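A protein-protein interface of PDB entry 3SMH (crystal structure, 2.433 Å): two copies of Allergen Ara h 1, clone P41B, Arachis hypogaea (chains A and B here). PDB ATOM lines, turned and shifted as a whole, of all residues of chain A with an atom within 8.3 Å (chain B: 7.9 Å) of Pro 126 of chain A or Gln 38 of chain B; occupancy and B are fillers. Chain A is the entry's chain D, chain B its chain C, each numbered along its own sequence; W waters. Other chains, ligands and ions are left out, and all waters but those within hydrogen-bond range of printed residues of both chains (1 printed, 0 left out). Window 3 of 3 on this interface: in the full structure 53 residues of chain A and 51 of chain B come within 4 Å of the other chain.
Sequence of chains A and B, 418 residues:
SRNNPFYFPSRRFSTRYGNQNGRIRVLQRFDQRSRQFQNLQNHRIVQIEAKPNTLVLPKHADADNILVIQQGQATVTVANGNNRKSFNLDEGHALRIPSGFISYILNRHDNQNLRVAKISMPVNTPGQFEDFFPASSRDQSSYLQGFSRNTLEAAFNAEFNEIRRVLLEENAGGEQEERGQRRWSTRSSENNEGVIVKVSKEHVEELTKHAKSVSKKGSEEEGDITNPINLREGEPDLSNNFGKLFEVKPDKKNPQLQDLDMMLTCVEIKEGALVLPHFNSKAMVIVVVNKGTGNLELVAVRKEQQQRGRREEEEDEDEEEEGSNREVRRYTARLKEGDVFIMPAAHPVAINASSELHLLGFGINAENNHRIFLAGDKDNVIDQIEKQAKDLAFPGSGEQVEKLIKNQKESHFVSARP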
ATOM      1  N   ARG A  29     -29.912  27.463  -0.292  1.00  0.00           N
ATOM      2  CA  ARG A  29     -28.632  28.160  -0.328  1.00  0.00           C
ATOM      3  C   ARG A  29     -28.431  28.877  -1.665  1.00  0.00           C
ATOM      4  O   ARG A  29     -28.658  28.308  -2.728  1.00  0.00           O
ATOM      5  CB  ARG A  29     -27.504  27.183  -0.100  1.00  0.00           C
ATOM      6  CG  ARG A  29     -27.602  26.474   1.216  1.00  0.00           C
ATOM      7  CD  ARG A  29     -26.473  25.495   1.345  1.00  0.00           C
ATOM      8  NE  ARG A  29     -25.246  26.079   0.833  1.00  0.00           N
ATOM      9  CZ  ARG A  29     -24.066  25.477   0.886  1.00  0.00           C
ATOM     10  NH1 ARG A  29     -23.959  24.277   1.445  1.00  0.00           N
ATOM     11  NH2 ARG A  29     -22.995  26.075   0.388  1.00  0.00           N
ATOM     12  N   ASP A  31     -25.809  29.930  -3.278  1.00  0.00           N
ATOM     13  CA  ASP A  31     -24.732  29.471  -4.145  1.00  0.00           C
ATOM     14  C   ASP A  31     -25.039  28.142  -4.835  1.00  0.00           C
ATOM     15  O   ASP A  31     -24.320  27.740  -5.751  1.00  0.00           O
ATOM     16  CB  ASP A  31     -23.390  29.418  -3.400  1.00  0.00           C
ATOM     17  CG  ASP A  31     -23.412  28.483  -2.197  1.00  0.00           C
ATOM     18  OD1 ASP A  31     -24.436  28.436  -1.477  1.00  0.00           O
ATOM     19  OD2 ASP A  31     -22.389  27.801  -1.979  1.00  0.00           O
ATOM     20  N   GLN A  32     -26.101  27.463  -4.403  1.00  0.00           N
ATOM     21  CA  GLN A  32     -26.551  26.260  -5.096  1.00  0.00           C
ATOM     22  C   GLN A  32     -27.307  26.619  -6.364  1.00  0.00           C
ATOM     23  O   GLN A  32     -27.223  25.910  -7.365  1.00  0.00           O
ATOM     24  CB  GLN A  32     -27.409  25.382  -4.187  1.00  0.00           C
ATOM     25  CG  GLN A  32     -26.603  24.653  -3.131  1.00  0.00           C
ATOM     26  CD  GLN A  32     -27.468  23.823  -2.208  1.00  0.00           C
ATOM     27  OE1 GLN A  32     -26.956  23.104  -1.341  1.00  0.00           O
ATOM     28  NE2 GLN A  32     -28.789  23.918  -2.385  1.00  0.00           N
ATOM     29  N   GLN A  38     -21.821  33.121  -4.867  1.00  0.00           N
ATOM     30  CA  GLN A  38     -20.887  32.531  -3.921  1.00  0.00           C
ATOM     31  C   GLN A  38     -20.672  33.437  -2.704  1.00  0.00           C
ATOM     32  O   GLN A  38     -20.553  32.956  -1.571  1.00  0.00           O
ATOM     33  CB  GLN A  38     -19.553  32.194  -4.586  1.00  0.00           C
ATOM     34  CG  GLN A  38     -18.862  31.026  -3.894  1.00  0.00           C
ATOM     35  CD  GLN A  38     -17.446  30.811  -4.380  1.00  0.00           C
ATOM     36  OE1 GLN A  38     -17.118  31.109  -5.533  1.00  0.00           O
ATOM     37  NE2 GLN A  38     -16.592  30.293  -3.498  1.00  0.00           N
ATOM     38  N   LEU A  40     -22.750  35.124  -1.180  1.00  0.00           N
ATOM     39  CA  LEU A  40     -23.936  35.113  -0.343  1.00  0.00           C
ATOM     40  C   LEU A  40     -24.118  33.731   0.256  1.00  0.00           C
ATOM     41  O   LEU A  40     -25.108  33.456   0.929  1.00  0.00           O
ATOM     42  CB  LEU A  40     -25.178  35.508  -1.150  1.00  0.00           C
ATOM     43  CG  LEU A  40     -25.190  36.948  -1.648  1.00  0.00           C
ATOM     44  CD1 LEU A  40     -26.358  37.202  -2.589  1.00  0.00           C
ATOM     45  CD2 LEU A  40     -25.204  37.907  -0.477  1.00  0.00           C
ATOM     46  N   GLN A  41     -23.145  32.869   0.000  1.00  0.00           N
ATOM     47  CA  GLN A  41     -23.201  31.486   0.429  1.00  0.00           C
ATOM     48  C   GLN A  41     -23.536  31.326   1.917  1.00  0.00           C
ATOM     49  O   GLN A  41     -24.257  30.406   2.303  1.00  0.00           O
ATOM     50  CB  GLN A  41     -21.866  30.820   0.119  1.00  0.00           C
ATOM     51  CG  GLN A  41     -21.572  29.577   0.914  1.00  0.00           C
ATOM     52  CD  GLN A  41     -20.129  29.156   0.756  1.00  0.00           C
ATOM     53  OE1 GLN A  41     -19.842  27.997   0.460  1.00  0.00           O
ATOM     54  NE2 GLN A  41     -19.209  30.100   0.948  1.00  0.00           N
ATOM     55  N   ASN A  42     -22.997  32.203   2.754  1.00  0.00           N
ATOM     56  CA  ASN A  42     -23.222  32.077   4.189  1.00  0.00           C
ATOM     57  C   ASN A  42     -24.415  32.887   4.716  1.00  0.00           C
ATOM     58  O   ASN A  42     -24.459  33.244   5.895  1.00  0.00           O
ATOM     59  CB  ASN A  42     -21.971  32.419   5.001  1.00  0.00           C
ATOM     60  CG  ASN A  42     -21.976  31.743   6.380  1.00  0.00           C
ATOM     61  OD1 ASN A  42     -22.243  30.541   6.492  1.00  0.00           O
ATOM     62  ND2 ASN A  42     -21.713  32.515   7.429  1.00  0.00           N
ATOM     63  N   HIS A  43     -25.374  33.181   3.840  1.00  0.00           N
ATOM     64  CA  HIS A  43     -26.576  33.876   4.241  1.00  0.00           C
ATOM     65  C   HIS A  43     -27.815  33.068   3.866  1.00  0.00           C
ATOM     66  O   HIS A  43     -28.049  32.775   2.689  1.00  0.00           O
ATOM     67  CB  HIS A  43     -26.609  35.269   3.636  1.00  0.00           C
ATOM     68  CG  HIS A  43     -25.556  36.178   4.180  1.00  0.00           C
ATOM     69  ND1 HIS A  43     -24.266  36.196   3.699  1.00  0.00           N
ATOM     70  CD2 HIS A  43     -25.594  37.084   5.186  1.00  0.00           C
ATOM     71  CE1 HIS A  43     -23.556  37.080   4.377  1.00  0.00           C
ATOM     72  NE2 HIS A  43     -24.341  37.633   5.286  1.00  0.00           N
ATOM     73  N   ARG A  44     -28.581  32.681   4.887  1.00  0.00           N
ATOM     74  CA  ARG A  44     -29.811  31.924   4.683  1.00  0.00           C
ATOM     75  C   ARG A  44     -30.982  32.781   5.113  1.00  0.00           C
ATOM     76  O   ARG A  44     -30.914  33.492   6.111  1.00  0.00           O
ATOM     77  CB  ARG A  44     -29.805  30.604   5.466  1.00  0.00           C
ATOM     78  CG  ARG A  44     -28.622  29.705   5.168  1.00  0.00           C
ATOM     79  CD  ARG A  44     -28.592  29.251   3.724  1.00  0.00           C
ATOM     80  NE  ARG A  44     -29.769  28.465   3.351  1.00  0.00           N
ATOM     81  CZ  ARG A  44     -29.953  27.180   3.661  1.00  0.00           C
ATOM     82  NH1 ARG A  44     -31.047  26.553   3.258  1.00  0.00           N
ATOM     83  NH2 ARG A  44     -29.052  26.506   4.376  1.00  0.00           N
ATOM     84  N   MET A 121     -26.670  33.557   9.564  1.00  0.00           N
ATOM     85  CA  MET A 121     -25.312  33.345   9.074  1.00  0.00           C
ATOM     86  C   MET A 121     -24.592  32.296   9.892  1.00  0.00           C
ATOM     87  O   MET A 121     -24.078  32.581  10.974  1.00  0.00           O
ATOM     88  CB  MET A 121     -24.508  34.639   9.070  1.00  0.00           C
ATOM     89  CG  MET A 121     -25.113  35.746   9.863  1.00  0.00           C
ATOM     90  SD  MET A 121     -25.755  37.070   8.829  1.00  0.00           S
ATOM     91  CE  MET A 121     -26.082  38.271  10.077  1.00  0.00           C
ATOM     92  N   PRO A 122     -24.559  31.072   9.367  1.00  0.00           N
ATOM     93  CA  PRO A 122     -23.936  29.921  10.028  1.00  0.00           C
ATOM     94  C   PRO A 122     -22.532  30.247  10.533  1.00  0.00           C
ATOM     95  O   PRO A 122     -21.796  31.006   9.899  1.00  0.00           O
ATOM     96  CB  PRO A 122     -23.893  28.881   8.913  1.00  0.00           C
ATOM     97  CG  PRO A 122     -25.112  29.208   8.082  1.00  0.00           C
ATOM     98  CD  PRO A 122     -25.187  30.712   8.087  1.00  0.00           C
ATOM     99  N   VAL A 123     -22.175  29.681  11.678  1.00  0.00           N
ATOM    100  CA  VAL A 123     -20.846  29.845  12.241  1.00  0.00           C
ATOM    101  C   VAL A 123     -19.865  28.725  11.862  1.00  0.00           C
ATOM    102  O   VAL A 123     -18.698  28.985  11.645  1.00  0.00           O
ATOM    103  CB  VAL A 123     -20.886  29.923  13.776  1.00  0.00           C
ATOM    104  CG1 VAL A 123     -19.467  29.852  14.320  1.00  0.00           C
ATOM    105  CG2 VAL A 123     -21.548  31.185  14.213  1.00  0.00           C
ATOM    106  N   ASN A 124     -20.338  27.488  11.787  1.00  0.00           N
ATOM    107  CA  ASN A 124     -19.430  26.348  11.617  1.00  0.00           C
ATOM    108  C   ASN A 124     -19.218  25.928  10.179  1.00  0.00           C
ATOM    109  O   ASN A 124     -18.096  25.760   9.726  1.00  0.00           O
ATOM    110  CB  ASN A 124     -19.916  25.136  12.434  1.00  0.00           C
ATOM    111  CG  ASN A 124     -19.925  25.411  13.917  1.00  0.00           C
ATOM    112  OD1 ASN A 124     -18.918  25.833  14.487  1.00  0.00           O
ATOM    113  ND2 ASN A 124     -21.074  25.216  14.545  1.00  0.00           N
ATOM    114  N   THR A 125     -20.316  25.745   9.471  1.00  0.00           N
ATOM    115  CA  THR A 125     -20.278  25.202   8.130  1.00  0.00           C
ATOM    116  C   THR A 125     -20.925  26.207   7.204  1.00  0.00           C
ATOM    117  O   THR A 125     -22.091  26.567   7.401  1.00  0.00           O
ATOM    118  CB  THR A 125     -21.086  23.885   8.068  1.00  0.00           C
ATOM    119  OG1 THR A 125     -20.587  22.970   9.051  1.00  0.00           O
ATOM    120  CG2 THR A 125     -20.973  23.263   6.683  1.00  0.00           C
ATOM    121  N   PRO A 126     -20.184  26.663   6.190  1.00  0.00           N
ATOM    122  CA  PRO A 126     -20.718  27.707   5.309  1.00  0.00           C
ATOM    123  C   PRO A 126     -22.079  27.352   4.748  1.00  0.00           C
ATOM    124  O   PRO A 126     -22.260  26.306   4.123  1.00  0.00           O
ATOM    125  CB  PRO A 126     -19.680  27.777   4.194  1.00  0.00           C
ATOM    126  CG  PRO A 126     -18.392  27.394   4.886  1.00  0.00           C
ATOM    127  CD  PRO A 126     -18.789  26.317   5.864  1.00  0.00           C
ATOM    128  N   GLY A 127     -23.045  28.224   5.000  1.00  0.00           N
ATOM    129  CA  GLY A 127     -24.391  28.023   4.514  1.00  0.00           C
ATOM    130  C   GLY A 127     -25.258  27.006   5.232  1.00  0.00           C
ATOM    131  O   GLY A 127     -26.402  26.816   4.840  1.00  0.00           O
ATOM    132  N   GLN A 128     -24.745  26.351   6.271  1.00  0.00           N
ATOM    133  CA  GLN A 128     -25.540  25.327   6.964  1.00  0.00           C
ATOM    134  C   GLN A 128     -25.604  25.579   8.459  1.00  0.00           C
ATOM    135  O   GLN A 128     -24.596  25.851   9.090  1.00  0.00           O
ATOM    136  CB  GLN A 128     -24.996  23.914   6.710  1.00  0.00           C
ATOM    137  CG  GLN A 128     -24.833  23.530   5.240  1.00  0.00           C
ATOM    138  CD  GLN A 128     -26.152  23.243   4.542  1.00  0.00           C
ATOM    139  OE1 GLN A 128     -27.235  23.425   5.116  1.00  0.00           O
ATOM    140  NE2 GLN A 128     -26.068  22.788   3.292  1.00  0.00           N
ATOM    141  N   PHE A 129     -26.803  25.484   9.027  1.00  0.00           N
ATOM    142  CA  PHE A 129     -26.961  25.633  10.461  1.00  0.00           C
ATOM    143  C   PHE A 129     -28.026  24.669  10.948  1.00  0.00           C
ATOM    144  O   PHE A 129     -28.766  24.120  10.143  1.00  0.00           O
ATOM    145  CB  PHE A 129     -27.332  27.078  10.817  1.00  0.00           C
ATOM    146  CG  PHE A 129     -28.704  27.478  10.369  1.00  0.00           C
ATOM    147  CD1 PHE A 129     -28.918  27.944   9.082  1.00  0.00           C
ATOM    148  CD2 PHE A 129     -29.786  27.382  11.234  1.00  0.00           C
ATOM    149  CE1 PHE A 129     -30.183  28.319   8.653  1.00  0.00           C
ATOM    150  CE2 PHE A 129     -31.058  27.752  10.817  1.00  0.00           C
ATOM    151  CZ  PHE A 129     -31.257  28.224   9.519  1.00  0.00           C
ATOM    152  N   ARG B  29      -4.960  18.544   7.401  1.00  0.00           N
ATOM    153  CA  ARG B  29      -5.877  19.656   7.198  1.00  0.00           C
ATOM    154  C   ARG B  29      -7.301  19.272   7.624  1.00  0.00           C
ATOM    155  O   ARG B  29      -7.814  18.211   7.268  1.00  0.00           O
ATOM    156  CB  ARG B  29      -5.854  20.091   5.742  1.00  0.00           C
ATOM    157  CG  ARG B  29      -4.506  20.572   5.285  1.00  0.00           C
ATOM    158  CD  ARG B  29      -4.553  20.935   3.835  1.00  0.00           C
ATOM    159  NE  ARG B  29      -5.765  21.692   3.554  1.00  0.00           N
ATOM    160  CZ  ARG B  29      -6.052  22.230   2.375  1.00  0.00           C
ATOM    161  NH1 ARG B  29      -5.209  22.092   1.356  1.00  0.00           N
ATOM    162  NH2 ARG B  29      -7.185  22.903   2.216  1.00  0.00           N
ATOM    163  N   PHE B  30      -7.934  20.145   8.395  1.00  0.00           N
ATOM    164  CA  PHE B  30      -9.239  19.852   8.956  1.00  0.00           C
ATOM    165  C   PHE B  30     -10.324  19.708   7.902  1.00  0.00           C
ATOM    166  O   PHE B  30     -11.245  18.905   8.061  1.00  0.00           O
ATOM    167  CB  PHE B  30      -9.647  20.934   9.944  1.00  0.00           C
ATOM    168  CG  PHE B  30      -8.828  20.951  11.191  1.00  0.00           C
ATOM    169  CD1 PHE B  30      -8.869  19.885  12.080  1.00  0.00           C
ATOM    170  CD2 PHE B  30      -8.020  22.040  11.483  1.00  0.00           C
ATOM    171  CE1 PHE B  30      -8.115  19.892  13.241  1.00  0.00           C
ATOM    172  CE2 PHE B  30      -7.262  22.060  12.647  1.00  0.00           C
ATOM    173  CZ  PHE B  30      -7.314  20.977  13.531  1.00  0.00           C
ATOM    174  N   ASP B  31     -10.228  20.494   6.838  1.00  0.00           N
ATOM    175  CA  ASP B  31     -11.243  20.444   5.806  1.00  0.00           C
ATOM    176  C   ASP B  31     -11.120  19.219   4.897  1.00  0.00           C
ATOM    177  O   ASP B  31     -12.032  18.908   4.144  1.00  0.00           O
ATOM    178  CB  ASP B  31     -11.272  21.748   4.999  1.00  0.00           C
ATOM    179  CG  ASP B  31      -9.965  22.039   4.304  1.00  0.00           C
ATOM    180  OD1 ASP B  31      -8.901  21.769   4.892  1.00  0.00           O
ATOM    181  OD2 ASP B  31     -10.010  22.549   3.168  1.00  0.00           O
ATOM    182  N   GLN B  32     -10.001  18.516   4.973  1.00  0.00           N
ATOM    183  CA  GLN B  32      -9.873  17.267   4.235  1.00  0.00           C
ATOM    184  C   GLN B  32     -10.657  16.152   4.919  1.00  0.00           C
ATOM    185  O   GLN B  32     -11.244  15.297   4.255  1.00  0.00           O
ATOM    186  CB  GLN B  32      -8.406  16.884   4.065  1.00  0.00           C
ATOM    187  CG  GLN B  32      -7.680  17.745   3.060  1.00  0.00           C
ATOM    188  CD  GLN B  32      -6.217  17.374   2.939  1.00  0.00           C
ATOM    189  OE1 GLN B  32      -5.492  17.930   2.110  1.00  0.00           O
ATOM    190  NE2 GLN B  32      -5.771  16.427   3.770  1.00  0.00           N
ATOM    191  N   SER B  34     -13.470  16.563   6.830  1.00  0.00           N
ATOM    192  CA  SER B  34     -14.878  16.817   6.570  1.00  0.00           C
ATOM    193  C   SER B  34     -15.107  18.258   6.138  1.00  0.00           C
ATOM    194  O   SER B  34     -14.368  19.167   6.531  1.00  0.00           O
ATOM    195  CB  SER B  34     -15.710  16.520   7.820  1.00  0.00           C
ATOM    196  OG  SER B  34     -17.025  17.032   7.677  1.00  0.00           O
ATOM    197  N   ARG B  35     -16.144  18.471   5.338  1.00  0.00           N
ATOM    198  CA  ARG B  35     -16.444  19.808   4.839  1.00  0.00           C
ATOM    199  C   ARG B  35     -17.074  20.705   5.896  1.00  0.00           C
ATOM    200  O   ARG B  35     -17.233  21.904   5.687  1.00  0.00           O
ATOM    201  CB  ARG B  35     -17.312  19.739   3.579  1.00  0.00           C
ATOM    202  CG  ARG B  35     -16.531  19.317   2.347  1.00  0.00           C
ATOM    203  CD  ARG B  35     -15.244  20.132   2.258  1.00  0.00           C
ATOM    204  NE  ARG B  35     -14.660  20.073   0.933  1.00  0.00           N
ATOM    205  CZ  ARG B  35     -14.614  21.058   0.040  1.00  0.00           C
ATOM    206  NH1 ARG B  35     -15.103  22.269   0.297  1.00  0.00           N
ATOM    207  NH2 ARG B  35     -14.047  20.812  -1.134  1.00  0.00           N
ATOM    208  N   GLN B  36     -17.428  20.128   7.039  1.00  0.00           N
ATOM    209  CA  GLN B  36     -17.981  20.936   8.113  1.00  0.00           C
ATOM    210  C   GLN B  36     -16.886  21.693   8.857  1.00  0.00           C
ATOM    211  O   GLN B  36     -17.153  22.463   9.787  1.00  0.00           O
ATOM    212  CB  GLN B  36     -18.826  20.093   9.073  1.00  0.00           C
ATOM    213  CG  GLN B  36     -18.105  18.924   9.678  1.00  0.00           C
ATOM    214  CD  GLN B  36     -19.041  18.000  10.427  1.00  0.00           C
ATOM    215  OE1 GLN B  36     -18.979  16.779  10.269  1.00  0.00           O
ATOM    216  NE2 GLN B  36     -19.913  18.577  11.254  1.00  0.00           N
ATOM    217  N   PHE B  37     -15.646  21.468   8.443  1.00  0.00           N
ATOM    218  CA  PHE B  37     -14.513  22.171   9.026  1.00  0.00           C
ATOM    219  C   PHE B  37     -13.910  23.146   8.017  1.00  0.00           C
ATOM    220  O   PHE B  37     -12.766  23.568   8.154  1.00  0.00           O
ATOM    221  CB  PHE B  37     -13.458  21.178   9.523  1.00  0.00           C
ATOM    222  CG  PHE B  37     -13.990  20.166  10.501  1.00  0.00           C
ATOM    223  CD1 PHE B  37     -14.887  20.547  11.485  1.00  0.00           C
ATOM    224  CD2 PHE B  37     -13.611  18.835  10.424  1.00  0.00           C
ATOM    225  CE1 PHE B  37     -15.388  19.624  12.375  1.00  0.00           C
ATOM    226  CE2 PHE B  37     -14.102  17.907  11.318  1.00  0.00           C
ATOM    227  CZ  PHE B  37     -14.993  18.298  12.298  1.00  0.00           C
ATOM    228  N   GLN B  38     -14.677  23.517   6.999  1.00  0.00           N
ATOM    229  CA  GLN B  38     -14.137  24.418   6.002  1.00  0.00           C
ATOM    230  C   GLN B  38     -13.643  25.714   6.654  1.00  0.00           C
ATOM    231  O   GLN B  38     -12.657  26.295   6.226  1.00  0.00           O
ATOM    232  CB  GLN B  38     -15.155  24.704   4.904  1.00  0.00           C
ATOM    233  CG  GLN B  38     -14.491  25.081   3.596  1.00  0.00           C
ATOM    234  CD  GLN B  38     -15.473  25.593   2.561  1.00  0.00           C
ATOM    235  OE1 GLN B  38     -16.651  25.224   2.562  1.00  0.00           O
ATOM    236  NE2 GLN B  38     -14.992  26.458   1.668  1.00  0.00           N
ATOM    237  N   ASN B  39     -14.321  26.153   7.705  1.00  0.00           N
ATOM    238  CA  ASN B  39     -13.943  27.386   8.383  1.00  0.00           C
ATOM    239  C   ASN B  39     -12.626  27.304   9.134  1.00  0.00           C
ATOM    240  O   ASN B  39     -12.085  28.333   9.541  1.00  0.00           O
ATOM    241  CB  ASN B  39     -15.042  27.850   9.343  1.00  0.00           C
ATOM    242  CG  ASN B  39     -16.190  28.558   8.629  1.00  0.00           C
ATOM    243  OD1 ASN B  39     -16.041  29.038   7.500  1.00  0.00           O
ATOM    244  ND2 ASN B  39     -17.339  28.628   9.292  1.00  0.00           N
ATOM    245  N   LEU B  40     -12.132  26.080   9.333  1.00  0.00           N
ATOM    246  CA  LEU B  40     -10.878  25.828  10.046  1.00  0.00           C
ATOM    247  C   LEU B  40      -9.789  25.451   9.049  1.00  0.00           C
ATOM    248  O   LEU B  40      -8.667  25.088   9.433  1.00  0.00           O
ATOM    249  CB  LEU B  40     -11.056  24.703  11.062  1.00  0.00           C
ATOM    250  CG  LEU B  40     -12.008  25.009  12.212  1.00  0.00           C
ATOM    251  CD1 LEU B  40     -12.280  23.768  13.035  1.00  0.00           C
ATOM    252  CD2 LEU B  40     -11.429  26.118  13.078  1.00  0.00           C
ATOM    253  N   GLN B  41     -10.131  25.546   7.766  1.00  0.00           N
ATOM    254  CA  GLN B  41      -9.225  25.158   6.695  1.00  0.00           C
ATOM    255  C   GLN B  41      -7.832  25.775   6.816  1.00  0.00           C
ATOM    256  O   GLN B  41      -6.829  25.118   6.530  1.00  0.00           O
ATOM    257  CB  GLN B  41      -9.843  25.533   5.358  1.00  0.00           C
ATOM    258  CG  GLN B  41      -8.887  25.612   4.212  1.00  0.00           C
ATOM    259  CD  GLN B  41      -9.507  26.311   3.017  1.00  0.00           C
ATOM    260  OE1 GLN B  41      -9.425  25.821   1.885  1.00  0.00           O
ATOM    261  NE2 GLN B  41     -10.129  27.466   3.261  1.00  0.00           N
ATOM    262  N   ASN B  42      -7.761  27.039   7.214  1.00  0.00           N
ATOM    263  CA  ASN B  42      -6.473  27.712   7.318  1.00  0.00           C
ATOM    264  C   ASN B  42      -5.842  27.638   8.700  1.00  0.00           C
ATOM    265  O   ASN B  42      -5.077  28.514   9.064  1.00  0.00           O
ATOM    266  CB  ASN B  42      -6.565  29.171   6.909  1.00  0.00           C
ATOM    267  CG  ASN B  42      -5.233  29.730   6.465  1.00  0.00           C
ATOM    268  OD1 ASN B  42      -4.525  29.113   5.651  1.00  0.00           O
ATOM    269  ND2 ASN B  42      -4.856  30.880   7.019  1.00  0.00           N
ATOM    270  N   HIS B  43      -6.186  26.618   9.478  1.00  0.00           N
ATOM    271  CA  HIS B  43      -5.535  26.388  10.761  1.00  0.00           C
ATOM    272  C   HIS B  43      -4.898  24.996  10.823  1.00  0.00           C
ATOM    273  O   HIS B  43      -5.564  23.983  10.707  1.00  0.00           O
ATOM    274  CB  HIS B  43      -6.517  26.607  11.903  1.00  0.00           C
ATOM    275  CG  HIS B  43      -6.956  28.026  12.041  1.00  0.00           C
ATOM    276  ND1 HIS B  43      -7.919  28.587  11.232  1.00  0.00           N
ATOM    277  CD2 HIS B  43      -6.541  29.012  12.871  1.00  0.00           C
ATOM    278  CE1 HIS B  43      -8.079  29.857  11.555  1.00  0.00           C
ATOM    279  NE2 HIS B  43      -7.254  30.142  12.544  1.00  0.00           N
ATOM    280  N   PRO B 126      -4.266  28.566   1.255  1.00  0.00           N
ATOM    281  CA  PRO B 126      -5.088  28.133   2.387  1.00  0.00           C
ATOM    282  C   PRO B 126      -4.702  26.732   2.869  1.00  0.00           C
ATOM    283  O   PRO B 126      -4.665  25.770   2.097  1.00  0.00           O
ATOM    284  CB  PRO B 126      -6.507  28.135   1.804  1.00  0.00           C
ATOM    285  CG  PRO B 126      -6.453  29.175   0.718  1.00  0.00           C
ATOM    286  CD  PRO B 126      -5.075  29.078   0.135  1.00  0.00           C
ATOM    287  N   MET B 284     -15.322  28.766  17.463  1.00  0.00           N
ATOM    288  CA  MET B 284     -14.986  27.385  17.144  1.00  0.00           C
ATOM    289  C   MET B 284     -13.650  27.100  17.818  1.00  0.00           C
ATOM    290  O   MET B 284     -12.715  27.895  17.696  1.00  0.00           O
ATOM    291  CB  MET B 284     -14.841  27.176  15.642  1.00  0.00           C
ATOM    292  CG  MET B 284     -16.041  27.610  14.862  1.00  0.00           C
ATOM    293  SD  MET B 284     -15.776  27.432  13.096  1.00  0.00           S
ATOM    294  CE  MET B 284     -15.680  25.628  12.984  1.00  0.00           C
ATOM    295  N   ILE B 364     -11.123  30.308  17.434  1.00  0.00           N
ATOM    296  CA  ILE B 364     -11.291  31.310  16.379  1.00  0.00           C
ATOM    297  C   ILE B 364     -12.708  31.883  16.376  1.00  0.00           C
ATOM    298  O   ILE B 364     -13.618  31.280  16.948  1.00  0.00           O
ATOM    299  CB  ILE B 364     -10.922  30.750  14.986  1.00  0.00           C
ATOM    300  CG1 ILE B 364     -11.997  29.809  14.477  1.00  0.00           C
ATOM    301  CG2 ILE B 364      -9.566  30.027  15.024  1.00  0.00           C
ATOM    302  CD1 ILE B 364     -11.866  29.532  13.004  1.00  0.00           C
HETATM  303  O   HOH W   1     -19.731  29.860   8.381  1.00  0.00           O
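ND2 of Asn 39 of chain B sits at hydrogen-bond distance from O of Val 123 of chain A, 2.7 Å away.
The side-chain amide nitrogen (ND2) of Asn 39 of chain B lies within hydrogen-bond range of the backbone carbonyl oxygen (O) of Asn 124 of chain A (3.0 Å).
SD of Met 284 of chain B sits close to OD1 of Asn 124 of chain A.
The side-chain sulfur (SD) of Met 284 of chain B lies close to the backbone carbonyl oxygen (O) of Val 123 of chain A, 3.6 Å away.
The backbone carbonyl oxygen (O) of Asn 124 of chain A lies close to the backbone carbonyl oxygen (O) of Gln 36 of chain B, 3.4 Å away.
OG of Ser 34 of chain B sits close to N of Gln 36 of chain B (3.2 Å).
The backbone NH (N) of Ile 364 of chain B is in hydrogen-bond range of the backbone carbonyl oxygen (O) of Met 284 of chain B (2.9 Å).
Among the printed residues, merely in contact across the chains: Thr 125 of chain A with Gln 36 of chain B (3.4 Å), Pro 126 of chain A with Gln 38 of chain B (3.6 Å) and Pro 126 of chain A with Asn 39 of chain B (3.9 Å).
Gln 38 of chain A touches none of the printed residues of chain B.
Printed residues of chain B within 4 Å of Asn 124 of chain A: Gln 36 (3.4 Å), Asn 39 (3.0 Å) and Met 284 (3.4 Å).
Pro 126 of chain A touches two residues of chain B.
Gln 32 of chain B touches none of the printed residues of chain A.
Of the printed residues of chain A, Gln 36 of chain B touches Asn 124 (3.4 Å) and Thr 125 (3.4 Å).
Of chain A, only Pro 126 comes within 4 Å of Gln 38 of chain B.
Of the printed residues of chain A, Met 284 of chain B touches Val 123 and Asn 124.
The nearest printed residue of chain B that does not touch Asn 124 of chain A is Gln 38 of chain B (4.9 Å).
Printed residues of chain A that touch a printed residue of chain B: Val 123, Asn 124, Thr 125 and Pro 126.
Hydrophobic or aromatic side chains of chain A within 4 Å of the printed part of chain B: Pro 126.
Of the 17 printed residues of chain B, 4 touch a printed residue of chain A.
Printed residues of chain B that touch a printed residue of chain A: Gln 36, Gln 38, Asn 39 and Met 284.
Hydrophobic or aromatic side chains of chain B that line the printed part of chain A: Met 284.
Along chain B the printed residues that touch a printed residue of chain A span positions 36 to 284.
Pro 126 of chain A touches Gln 38 of chain B, but with the chains exchanged Gln 38 of chain A does not touch Pro 126 of chain B (11.0 Å).
Positions printed for both chains: 29, 31, 32, 38, 40, 41, 42, 43 and 126.
Water W1 lies within hydrogen-bond range of the backbone carbonyl oxygen of Pro 122 of chain A, the side-chain amide nitrogen of Asn 39 of chain B and the side-chain amide oxygen of Asn 42 of chain A.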
